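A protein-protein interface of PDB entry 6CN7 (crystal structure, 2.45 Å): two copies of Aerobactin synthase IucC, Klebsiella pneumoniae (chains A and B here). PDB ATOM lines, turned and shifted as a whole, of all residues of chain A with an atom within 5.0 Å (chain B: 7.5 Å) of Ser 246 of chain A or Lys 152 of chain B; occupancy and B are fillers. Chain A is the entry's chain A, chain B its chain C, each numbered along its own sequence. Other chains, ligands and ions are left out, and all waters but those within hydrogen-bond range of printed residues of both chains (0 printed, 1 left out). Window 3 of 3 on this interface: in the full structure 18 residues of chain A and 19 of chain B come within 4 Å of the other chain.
NH2 of Arg 157 of chain B is in salt-bridge range of OE2 of Glu 153 of chain B, 2.7 Å away.
The side-chain hydroxyl (OG) of Ser 232 of chain A is in hydrogen-bond range of the backbone carbonyl oxygen (O) of Trp 227 of chain A.
NE2 of His 169 of chain A is in hydrogen-bond range of OG of Ser 246 of chain A (2.9 Å).
The side-chain carboxylate of Glu 156 of chain B is in salt-bridge range of the side-chain amino group of Lys 152 of chain B (2.7 Å).
The backbone carbonyl oxygen (O) of Ser 232 of chain A is in hydrogen-bond range of the backbone NH (N) of Lys 152 of chain B (2.9 Å).
OE1 of Glu 153 of chain B lies within hydrogen-bond range of NE1 of Trp 227 of chain A.
No position is printed for both chains.
Of the 9 pairs that touch across the chains among the printed residues, none has its exchanged pair printed and touching as well.
Of the 13 printed residues of chain B, 6 touch a printed residue of chain A.
Hydrophobic or aromatic side chains of chain B within 4 Å of the printed part of chain A: Leu 106.
Of the 13 printed residues of chain A, 5 touch a printed residue of chain B.
Hydrophobic or aromatic side chains of chain A that line the printed part of chain B: Trp 227, Leu 233 and Ile 236.
Among the printed residues, 9 pairs touch across the chains.
Among the printed residues, no Asp or Glu carboxylate lies within 4 Å of a Lys or Arg side-chain nitrogen of the other chain.
Ser 246 of chain A touches just one residue of chain B: Lys 152.
Of chain A, only Ser 232 (2.9 Å) and Ser 246 (3.8 Å) come within 4 Å of Lys 152 of chain B.
Printed residues of chain A within 4 Å of Gly 151 of chain B: Ser 232 and Leu 233.
Of the printed residues of chain B, Trp 227 of chain A touches Glu 153.
Of the printed residues of chain B, Ile 236 of chain A touches Leu 106 (3.7 Å).
Printed residues of chain B within 4 Å of Leu 233 of chain A: Gly 149 (3.6 Å), Trp 150 (3.7 Å) and Gly 151 (3.97 Å).
Of the printed residues of chain A, Leu 106 of chain B touches Ile 236.
Met 244 of chain A touches none of the printed residues of chain B.
The nearest residue of chain B that does not touch Ser 246 of chain A is Glu 153 of chain B (5.4 Å).
The nearest residue of chain A that does not touch Lys 152 of chain B is Leu 239 of chain A (4.1 Å).
The nearest printed residue of chain A that does not touch Leu 106 of chain B is Leu 239 of chain A (4.8 Å).
Among the printed residues, merely in contact across the chains: Ser 232 of chain A with Gly 151 of chain B, Leu 233 of chain A with Gly 149 of chain B, Ile 236 of chain A with Leu 106 of chain B, Leu 233 of chain A with Trp 150 of chain B, Ser 246 of chain A with Lys 152 of chain B, Ser 232 of chain A with Glu 153 of chain B and Leu 233 of chain A with Gly 151 of chain B.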
ATOM      1  N   HIS A 169      -2.655  -1.540  12.217  1.00  0.00           N
ATOM      2  CA  HIS A 169      -2.483  -0.768  13.435  1.00  0.00           C
ATOM      3  C   HIS A 169      -2.279  -1.723  14.606  1.00  0.00           C
ATOM      4  O   HIS A 169      -2.831  -2.827  14.630  1.00  0.00           O
ATOM      5  CB  HIS A 169      -3.700   0.124  13.674  1.00  0.00           C
ATOM      6  CG  HIS A 169      -3.481   1.192  14.697  1.00  0.00           C
ATOM      7  ND1 HIS A 169      -2.882   2.396  14.397  1.00  0.00           N
ATOM      8  CD2 HIS A 169      -3.790   1.243  16.013  1.00  0.00           C
ATOM      9  CE1 HIS A 169      -2.828   3.142  15.486  1.00  0.00           C
ATOM     10  NE2 HIS A 169      -3.373   2.464  16.480  1.00  0.00           N
ATOM     11  N   TRP A 170      -1.474  -1.296  15.577  1.00  0.00           N
ATOM     12  CA  TRP A 170      -1.076  -2.153  16.688  1.00  0.00           C
ATOM     13  C   TRP A 170      -1.453  -1.511  18.014  1.00  0.00           C
ATOM     14  O   TRP A 170      -1.157  -0.334  18.249  1.00  0.00           O
ATOM     15  CB  TRP A 170       0.426  -2.437  16.643  1.00  0.00           C
ATOM     16  CG  TRP A 170       0.798  -3.311  15.497  1.00  0.00           C
ATOM     17  CD1 TRP A 170       1.158  -2.911  14.245  1.00  0.00           C
ATOM     18  CD2 TRP A 170       0.828  -4.742  15.486  1.00  0.00           C
ATOM     19  NE1 TRP A 170       1.417  -4.004  13.454  1.00  0.00           N
ATOM     20  CE2 TRP A 170       1.221  -5.141  14.194  1.00  0.00           C
ATOM     21  CE3 TRP A 170       0.563  -5.725  16.444  1.00  0.00           C
ATOM     22  CZ2 TRP A 170       1.357  -6.480  13.836  1.00  0.00           C
ATOM     23  CZ3 TRP A 170       0.700  -7.054  16.088  1.00  0.00           C
ATOM     24  CH2 TRP A 170       1.093  -7.418  14.796  1.00  0.00           C
ATOM     25  N   LEU A 171      -2.102  -2.291  18.872  1.00  0.00           N
ATOM     26  CA  LEU A 171      -2.470  -1.877  20.217  1.00  0.00           C
ATOM     27  C   LEU A 171      -1.697  -2.694  21.242  1.00  0.00           C
ATOM     28  O   LEU A 171      -1.102  -3.730  20.934  1.00  0.00           O
ATOM     29  CB  LEU A 171      -3.976  -2.044  20.453  1.00  0.00           C
ATOM     30  CG  LEU A 171      -4.932  -1.214  19.596  1.00  0.00           C
ATOM     31  CD1 LEU A 171      -6.371  -1.534  19.970  1.00  0.00           C
ATOM     32  CD2 LEU A 171      -4.653   0.269  19.753  1.00  0.00           C
ATOM     33  N   TRP A 227      -9.631   0.584  13.372  1.00  0.00           N
ATOM     34  CA  TRP A 227      -9.071   1.584  14.278  1.00  0.00           C
ATOM     35  C   TRP A 227      -9.590   2.976  13.945  1.00  0.00           C
ATOM     36  O   TRP A 227      -9.964   3.741  14.843  1.00  0.00           O
ATOM     37  CB  TRP A 227      -7.546   1.574  14.211  1.00  0.00           C
ATOM     38  CG  TRP A 227      -6.940   2.776  14.868  1.00  0.00           C
ATOM     39  CD1 TRP A 227      -6.369   3.850  14.249  1.00  0.00           C
ATOM     40  CD2 TRP A 227      -6.864   3.036  16.272  1.00  0.00           C
ATOM     41  NE1 TRP A 227      -5.936   4.761  15.183  1.00  0.00           N
ATOM     42  CE2 TRP A 227      -6.228   4.283  16.433  1.00  0.00           C
ATOM     43  CE3 TRP A 227      -7.270   2.334  17.410  1.00  0.00           C
ATOM     44  CZ2 TRP A 227      -5.987   4.841  17.686  1.00  0.00           C
ATOM     45  CZ3 TRP A 227      -7.031   2.887  18.653  1.00  0.00           C
ATOM     46  CH2 TRP A 227      -6.395   4.129  18.782  1.00  0.00           C
ATOM     47  N   SER A 232     -10.757   3.801  17.746  1.00  0.00           N
ATOM     48  CA  SER A 232     -10.254   5.102  18.175  1.00  0.00           C
ATOM     49  C   SER A 232     -11.353   5.969  18.775  1.00  0.00           C
ATOM     50  O   SER A 232     -11.050   6.922  19.501  1.00  0.00           O
ATOM     51  CB  SER A 232      -9.607   5.835  17.001  1.00  0.00           C
ATOM     52  OG  SER A 232     -10.582   6.217  16.043  1.00  0.00           O
ATOM     53  N   LEU A 233     -12.616   5.663  18.487  1.00  0.00           N
ATOM     54  CA  LEU A 233     -13.753   6.416  18.999  1.00  0.00           C
ATOM     55  C   LEU A 233     -14.532   5.654  20.061  1.00  0.00           C
ATOM     56  O   LEU A 233     -14.729   6.161  21.170  1.00  0.00           O
ATOM     57  CB  LEU A 233     -14.684   6.790  17.834  1.00  0.00           C
ATOM     58  CG  LEU A 233     -15.972   7.540  18.177  1.00  0.00           C
ATOM     59  CD1 LEU A 233     -15.662   8.873  18.834  1.00  0.00           C
ATOM     60  CD2 LEU A 233     -16.816   7.737  16.924  1.00  0.00           C
ATOM     61  N   ILE A 236     -12.455   5.193  23.190  1.00  0.00           N
ATOM     62  CA  ILE A 236     -11.636   6.351  23.533  1.00  0.00           C
ATOM     63  C   ILE A 236     -11.451   6.454  25.041  1.00  0.00           C
ATOM     64  O   ILE A 236     -10.407   6.919  25.515  1.00  0.00           O
ATOM     65  CB  ILE A 236     -12.263   7.633  22.947  1.00  0.00           C
ATOM     66  CG1 ILE A 236     -11.309   8.817  23.116  1.00  0.00           C
ATOM     67  CG2 ILE A 236     -13.611   7.925  23.606  1.00  0.00           C
ATOM     68  CD1 ILE A 236     -11.723  10.051  22.339  1.00  0.00           C
ATOM     69  N   LEU A 239      -8.631   4.295  26.003  1.00  0.00           N
ATOM     70  CA  LEU A 239      -7.358   4.844  25.544  1.00  0.00           C
ATOM     71  C   LEU A 239      -6.890   5.987  26.435  1.00  0.00           C
ATOM     72  O   LEU A 239      -5.690   6.121  26.702  1.00  0.00           O
ATOM     73  CB  LEU A 239      -7.484   5.312  24.096  1.00  0.00           C
ATOM     74  CG  LEU A 239      -7.737   4.210  23.069  1.00  0.00           C
ATOM     75  CD1 LEU A 239      -8.153   4.814  21.741  1.00  0.00           C
ATOM     76  CD2 LEU A 239      -6.496   3.346  22.903  1.00  0.00           C
ATOM     77  N   MET A 244      -5.720   0.676  27.539  1.00  0.00           N
ATOM     78  CA  MET A 244      -5.274   0.275  26.214  1.00  0.00           C
ATOM     79  C   MET A 244      -4.373   1.370  25.666  1.00  0.00           C
ATOM     80  O   MET A 244      -4.607   2.554  25.920  1.00  0.00           O
ATOM     81  CB  MET A 244      -6.456   0.052  25.268  1.00  0.00           C
ATOM     82  CG  MET A 244      -7.231  -1.232  25.503  1.00  0.00           C
ATOM     83  SD  MET A 244      -8.811  -1.267  24.623  1.00  0.00           S
ATOM     84  CE  MET A 244      -8.469  -0.258  23.180  1.00  0.00           C
ATOM     85  N   VAL A 245      -3.353   0.972  24.911  1.00  0.00           N
ATOM     86  CA  VAL A 245      -2.359   1.904  24.392  1.00  0.00           C
ATOM     87  C   VAL A 245      -2.285   1.749  22.881  1.00  0.00           C
ATOM     88  O   VAL A 245      -2.192   0.626  22.371  1.00  0.00           O
ATOM     89  CB  VAL A 245      -0.975   1.680  25.032  1.00  0.00           C
ATOM     90  CG1 VAL A 245       0.058   2.633  24.443  1.00  0.00           C
ATOM     91  CG2 VAL A 245      -1.062   1.852  26.541  1.00  0.00           C
ATOM     92  N   SER A 246      -2.325   2.874  22.172  1.00  0.00           N
ATOM     93  CA  SER A 246      -2.217   2.892  20.720  1.00  0.00           C
ATOM     94  C   SER A 246      -0.757   3.097  20.333  1.00  0.00           C
ATOM     95  O   SER A 246      -0.166   4.133  20.655  1.00  0.00           O
ATOM     96  CB  SER A 246      -3.097   3.999  20.140  1.00  0.00           C
ATOM     97  OG  SER A 246      -2.812   4.218  18.774  1.00  0.00           O
ATOM     98  N   LEU A 247      -0.182   2.113  19.643  1.00  0.00           N
ATOM     99  CA  LEU A 247       1.228   2.165  19.275  1.00  0.00           C
ATOM    100  C   LEU A 247       1.452   2.731  17.883  1.00  0.00           C
ATOM    101  O   LEU A 247       2.499   3.340  17.633  1.00  0.00           O
ATOM    102  CB  LEU A 247       1.847   0.767  19.356  1.00  0.00           C
ATOM    103  CG  LEU A 247       2.261   0.293  20.751  1.00  0.00           C
ATOM    104  CD1 LEU A 247       1.081   0.283  21.706  1.00  0.00           C
ATOM    105  CD2 LEU A 247       2.891  -1.086  20.674  1.00  0.00           C
ATOM    106  N   GLY A 248       0.505   2.546  16.979  1.00  0.00           N
ATOM    107  CA  GLY A 248       0.625   3.015  15.616  1.00  0.00           C
ATOM    108  C   GLY A 248       0.685   1.857  14.638  1.00  0.00           C
ATOM    109  O   GLY A 248       0.445   0.695  14.977  1.00  0.00           O
ATOM    110  N   ALA B 103     -12.214  13.066  25.081  1.00  0.00           N
ATOM    111  CA  ALA B 103     -11.517  13.826  24.050  1.00  0.00           C
ATOM    112  C   ALA B 103     -10.889  15.086  24.626  1.00  0.00           C
ATOM    113  O   ALA B 103      -9.824  15.517  24.168  1.00  0.00           O
ATOM    114  CB  ALA B 103     -12.479  14.184  22.917  1.00  0.00           C
ATOM    115  N   LEU B 106      -7.773  13.947  26.696  1.00  0.00           N
ATOM    116  CA  LEU B 106      -6.676  13.639  25.785  1.00  0.00           C
ATOM    117  C   LEU B 106      -5.964  14.911  25.347  1.00  0.00           C
ATOM    118  O   LEU B 106      -4.731  14.987  25.371  1.00  0.00           O
ATOM    119  CB  LEU B 106      -7.202  12.867  24.572  1.00  0.00           C
ATOM    120  CG  LEU B 106      -7.565  11.398  24.811  1.00  0.00           C
ATOM    121  CD1 LEU B 106      -8.289  10.827  23.605  1.00  0.00           C
ATOM    122  CD2 LEU B 106      -6.326  10.568  25.119  1.00  0.00           C
ATOM    123  N   GLY B 149     -18.053  12.652  16.841  1.00  0.00           N
ATOM    124  CA  GLY B 149     -17.558  11.666  15.904  1.00  0.00           C
ATOM    125  C   GLY B 149     -16.051  11.556  15.803  1.00  0.00           C
ATOM    126  O   GLY B 149     -15.561  10.620  15.160  1.00  0.00           O
ATOM    127  N   TRP B 150     -15.300  12.467  16.417  1.00  0.00           N
ATOM    128  CA  TRP B 150     -13.845  12.473  16.311  1.00  0.00           C
ATOM    129  C   TRP B 150     -13.242  11.568  17.380  1.00  0.00           C
ATOM    130  O   TRP B 150     -13.419  11.811  18.578  1.00  0.00           O
ATOM    131  CB  TRP B 150     -13.294  13.891  16.452  1.00  0.00           C
ATOM    132  CG  TRP B 150     -13.555  14.772  15.270  1.00  0.00           C
ATOM    133  CD1 TRP B 150     -14.684  14.811  14.504  1.00  0.00           C
ATOM    134  CD2 TRP B 150     -12.659  15.741  14.713  1.00  0.00           C
ATOM    135  NE1 TRP B 150     -14.548  15.748  13.508  1.00  0.00           N
ATOM    136  CE2 TRP B 150     -13.313  16.334  13.615  1.00  0.00           C
ATOM    137  CE3 TRP B 150     -11.368  16.168  15.040  1.00  0.00           C
ATOM    138  CZ2 TRP B 150     -12.719  17.328  12.842  1.00  0.00           C
ATOM    139  CZ3 TRP B 150     -10.780  17.155  14.271  1.00  0.00           C
ATOM    140  CH2 TRP B 150     -11.455  17.723  13.185  1.00  0.00           C
ATOM    141  N   GLY B 151     -12.531  10.530  16.943  1.00  0.00           N
ATOM    142  CA  GLY B 151     -11.788   9.668  17.837  1.00  0.00           C
ATOM    143  C   GLY B 151     -10.354  10.135  18.008  1.00  0.00           C
ATOM    144  O   GLY B 151      -9.950  11.201  17.541  1.00  0.00           O
ATOM    145  N   LYS B 152      -9.567   9.300  18.693  1.00  0.00           N
ATOM    146  CA  LYS B 152      -8.180   9.661  18.972  1.00  0.00           C
ATOM    147  C   LYS B 152      -7.415   9.955  17.688  1.00  0.00           C
ATOM    148  O   LYS B 152      -6.650  10.926  17.621  1.00  0.00           O
ATOM    149  CB  LYS B 152      -7.494   8.547  19.767  1.00  0.00           C
ATOM    150  CG  LYS B 152      -6.053   8.863  20.160  1.00  0.00           C
ATOM    151  CD  LYS B 152      -5.525   7.884  21.206  1.00  0.00           C
ATOM    152  CE  LYS B 152      -4.054   8.134  21.526  1.00  0.00           C
ATOM    153  NZ  LYS B 152      -3.152   7.747  20.403  1.00  0.00           N
ATOM    154  N   GLU B 153      -7.608   9.133  16.653  1.00  0.00           N
ATOM    155  CA  GLU B 153      -6.917   9.361  15.387  1.00  0.00           C
ATOM    156  C   GLU B 153      -7.303  10.708  14.790  1.00  0.00           C
ATOM    157  O   GLU B 153      -6.436  11.518  14.436  1.00  0.00           O
ATOM    158  CB  GLU B 153      -7.234   8.230  14.407  1.00  0.00           C
ATOM    159  CG  GLU B 153      -6.311   8.174  13.196  1.00  0.00           C
ATOM    160  CD  GLU B 153      -4.946   7.607  13.526  1.00  0.00           C
ATOM    161  OE1 GLU B 153      -4.714   7.253  14.701  1.00  0.00           O
ATOM    162  OE2 GLU B 153      -4.104   7.512  12.608  1.00  0.00           O
ATOM    163  N   ALA B 154      -8.607  10.968  14.670  1.00  0.00           N
ATOM    164  CA  ALA B 154      -9.065  12.222  14.082  1.00  0.00           C
ATOM    165  C   ALA B 154      -8.567  13.421  14.876  1.00  0.00           C
ATOM    166  O   ALA B 154      -8.149  14.431  14.296  1.00  0.00           O
ATOM    167  CB  ALA B 154     -10.590  12.233  14.000  1.00  0.00           C
ATOM    168  N   LEU B 155      -8.604  13.330  16.206  1.00  0.00           N
ATOM    169  CA  LEU B 155      -8.167  14.445  17.040  1.00  0.00           C
ATOM    170  C   LEU B 155      -6.691  14.744  16.821  1.00  0.00           C
ATOM    171  O   LEU B 155      -6.304  15.897  16.594  1.00  0.00           O
ATOM    172  CB  LEU B 155      -8.436  14.129  18.512  1.00  0.00           C
ATOM    173  CG  LEU B 155      -9.905  14.003  18.911  1.00  0.00           C
ATOM    174  CD1 LEU B 155     -10.039  13.266  20.232  1.00  0.00           C
ATOM    175  CD2 LEU B 155     -10.536  15.379  18.994  1.00  0.00           C
ATOM    176  N   GLU B 156      -5.849  13.712  16.884  1.00  0.00           N
ATOM    177  CA  GLU B 156      -4.408  13.921  16.787  1.00  0.00           C
ATOM    178  C   GLU B 156      -4.004  14.468  15.424  1.00  0.00           C
ATOM    179  O   GLU B 156      -3.025  15.214  15.322  1.00  0.00           O
ATOM    180  CB  GLU B 156      -3.676  12.612  17.072  1.00  0.00           C
ATOM    181  CG  GLU B 156      -3.800  12.146  18.511  1.00  0.00           C
ATOM    182  CD  GLU B 156      -3.092  10.832  18.765  1.00  0.00           C
ATOM    183  OE1 GLU B 156      -2.666  10.184  17.783  1.00  0.00           O
ATOM    184  OE2 GLU B 156      -2.956  10.448  19.945  1.00  0.00           O
ATOM    185  N   ARG B 157      -4.740  14.120  14.368  1.00  0.00           N
ATOM    186  CA  ARG B 157      -4.332  14.525  13.027  1.00  0.00           C
ATOM    187  C   ARG B 157      -4.753  15.953  12.697  1.00  0.00           C
ATOM    188  O   ARG B 157      -4.015  16.672  12.016  1.00  0.00           O
ATOM    189  CB  ARG B 157      -4.902  13.558  11.990  1.00  0.00           C
ATOM    190  CG  ARG B 157      -4.167  12.232  11.927  1.00  0.00           C
ATOM    191  CD  ARG B 157      -4.709  11.355  10.819  1.00  0.00           C
ATOM    192  NE  ARG B 157      -4.007  10.077  10.738  1.00  0.00           N
ATOM    193  CZ  ARG B 157      -4.374   9.070   9.953  1.00  0.00           C
ATOM    194  NH1 ARG B 157      -5.443   9.183   9.177  1.00  0.00           N
ATOM    195  NH2 ARG B 157      -3.672   7.944   9.947  1.00  0.00           N
ATOM    196  N   TYR B 158      -5.924  16.391  13.170  1.00  0.00           N
ATOM    197  CA  TYR B 158      -6.519  17.637  12.697  1.00  0.00           C
ATOM    198  C   TYR B 158      -6.843  18.653  13.785  1.00  0.00           C
ATOM    199  O   TYR B 158      -7.134  19.807  13.450  1.00  0.00           O
ATOM    200  CB  TYR B 158      -7.801  17.329  11.905  1.00  0.00           C
ATOM    201  CG  TYR B 158      -7.603  16.217  10.901  1.00  0.00           C
ATOM    202  CD1 TYR B 158      -6.665  16.339   9.887  1.00  0.00           C
ATOM    203  CD2 TYR B 158      -8.340  15.041  10.975  1.00  0.00           C
ATOM    204  CE1 TYR B 158      -6.465  15.327   8.969  1.00  0.00           C
ATOM    205  CE2 TYR B 158      -8.149  14.022  10.059  1.00  0.00           C
ATOM    206  CZ  TYR B 158      -7.211  14.173   9.057  1.00  0.00           C
ATOM    207  OH  TYR B 158      -7.012  13.168   8.138  1.00  0.00           O
ATOM    208  N   TYR B 162      -2.828  19.330  19.142  1.00  0.00           N
ATOM    209  CA  TYR B 162      -1.728  18.439  18.789  1.00  0.00           C
ATOM    210  C   TYR B 162      -0.774  19.058  17.775  1.00  0.00           C
ATOM    211  O   TYR B 162       0.334  18.542  17.593  1.00  0.00           O
ATOM    212  CB  TYR B 162      -2.277  17.116  18.245  1.00  0.00           C
ATOM    213  CG  TYR B 162      -3.213  16.424  19.211  1.00  0.00           C
ATOM    214  CD1 TYR B 162      -2.735  15.524  20.155  1.00  0.00           C
ATOM    215  CD2 TYR B 162      -4.576  16.679  19.183  1.00  0.00           C
ATOM    216  CE1 TYR B 162      -3.591  14.898  21.041  1.00  0.00           C
ATOM    217  CE2 TYR B 162      -5.437  16.059  20.063  1.00  0.00           C
ATOM    218  CZ  TYR B 162      -4.940  15.168  20.989  1.00  0.00           C
ATOM    219  OH  TYR B 162      -5.797  14.551  21.868  1.00  0.00           O
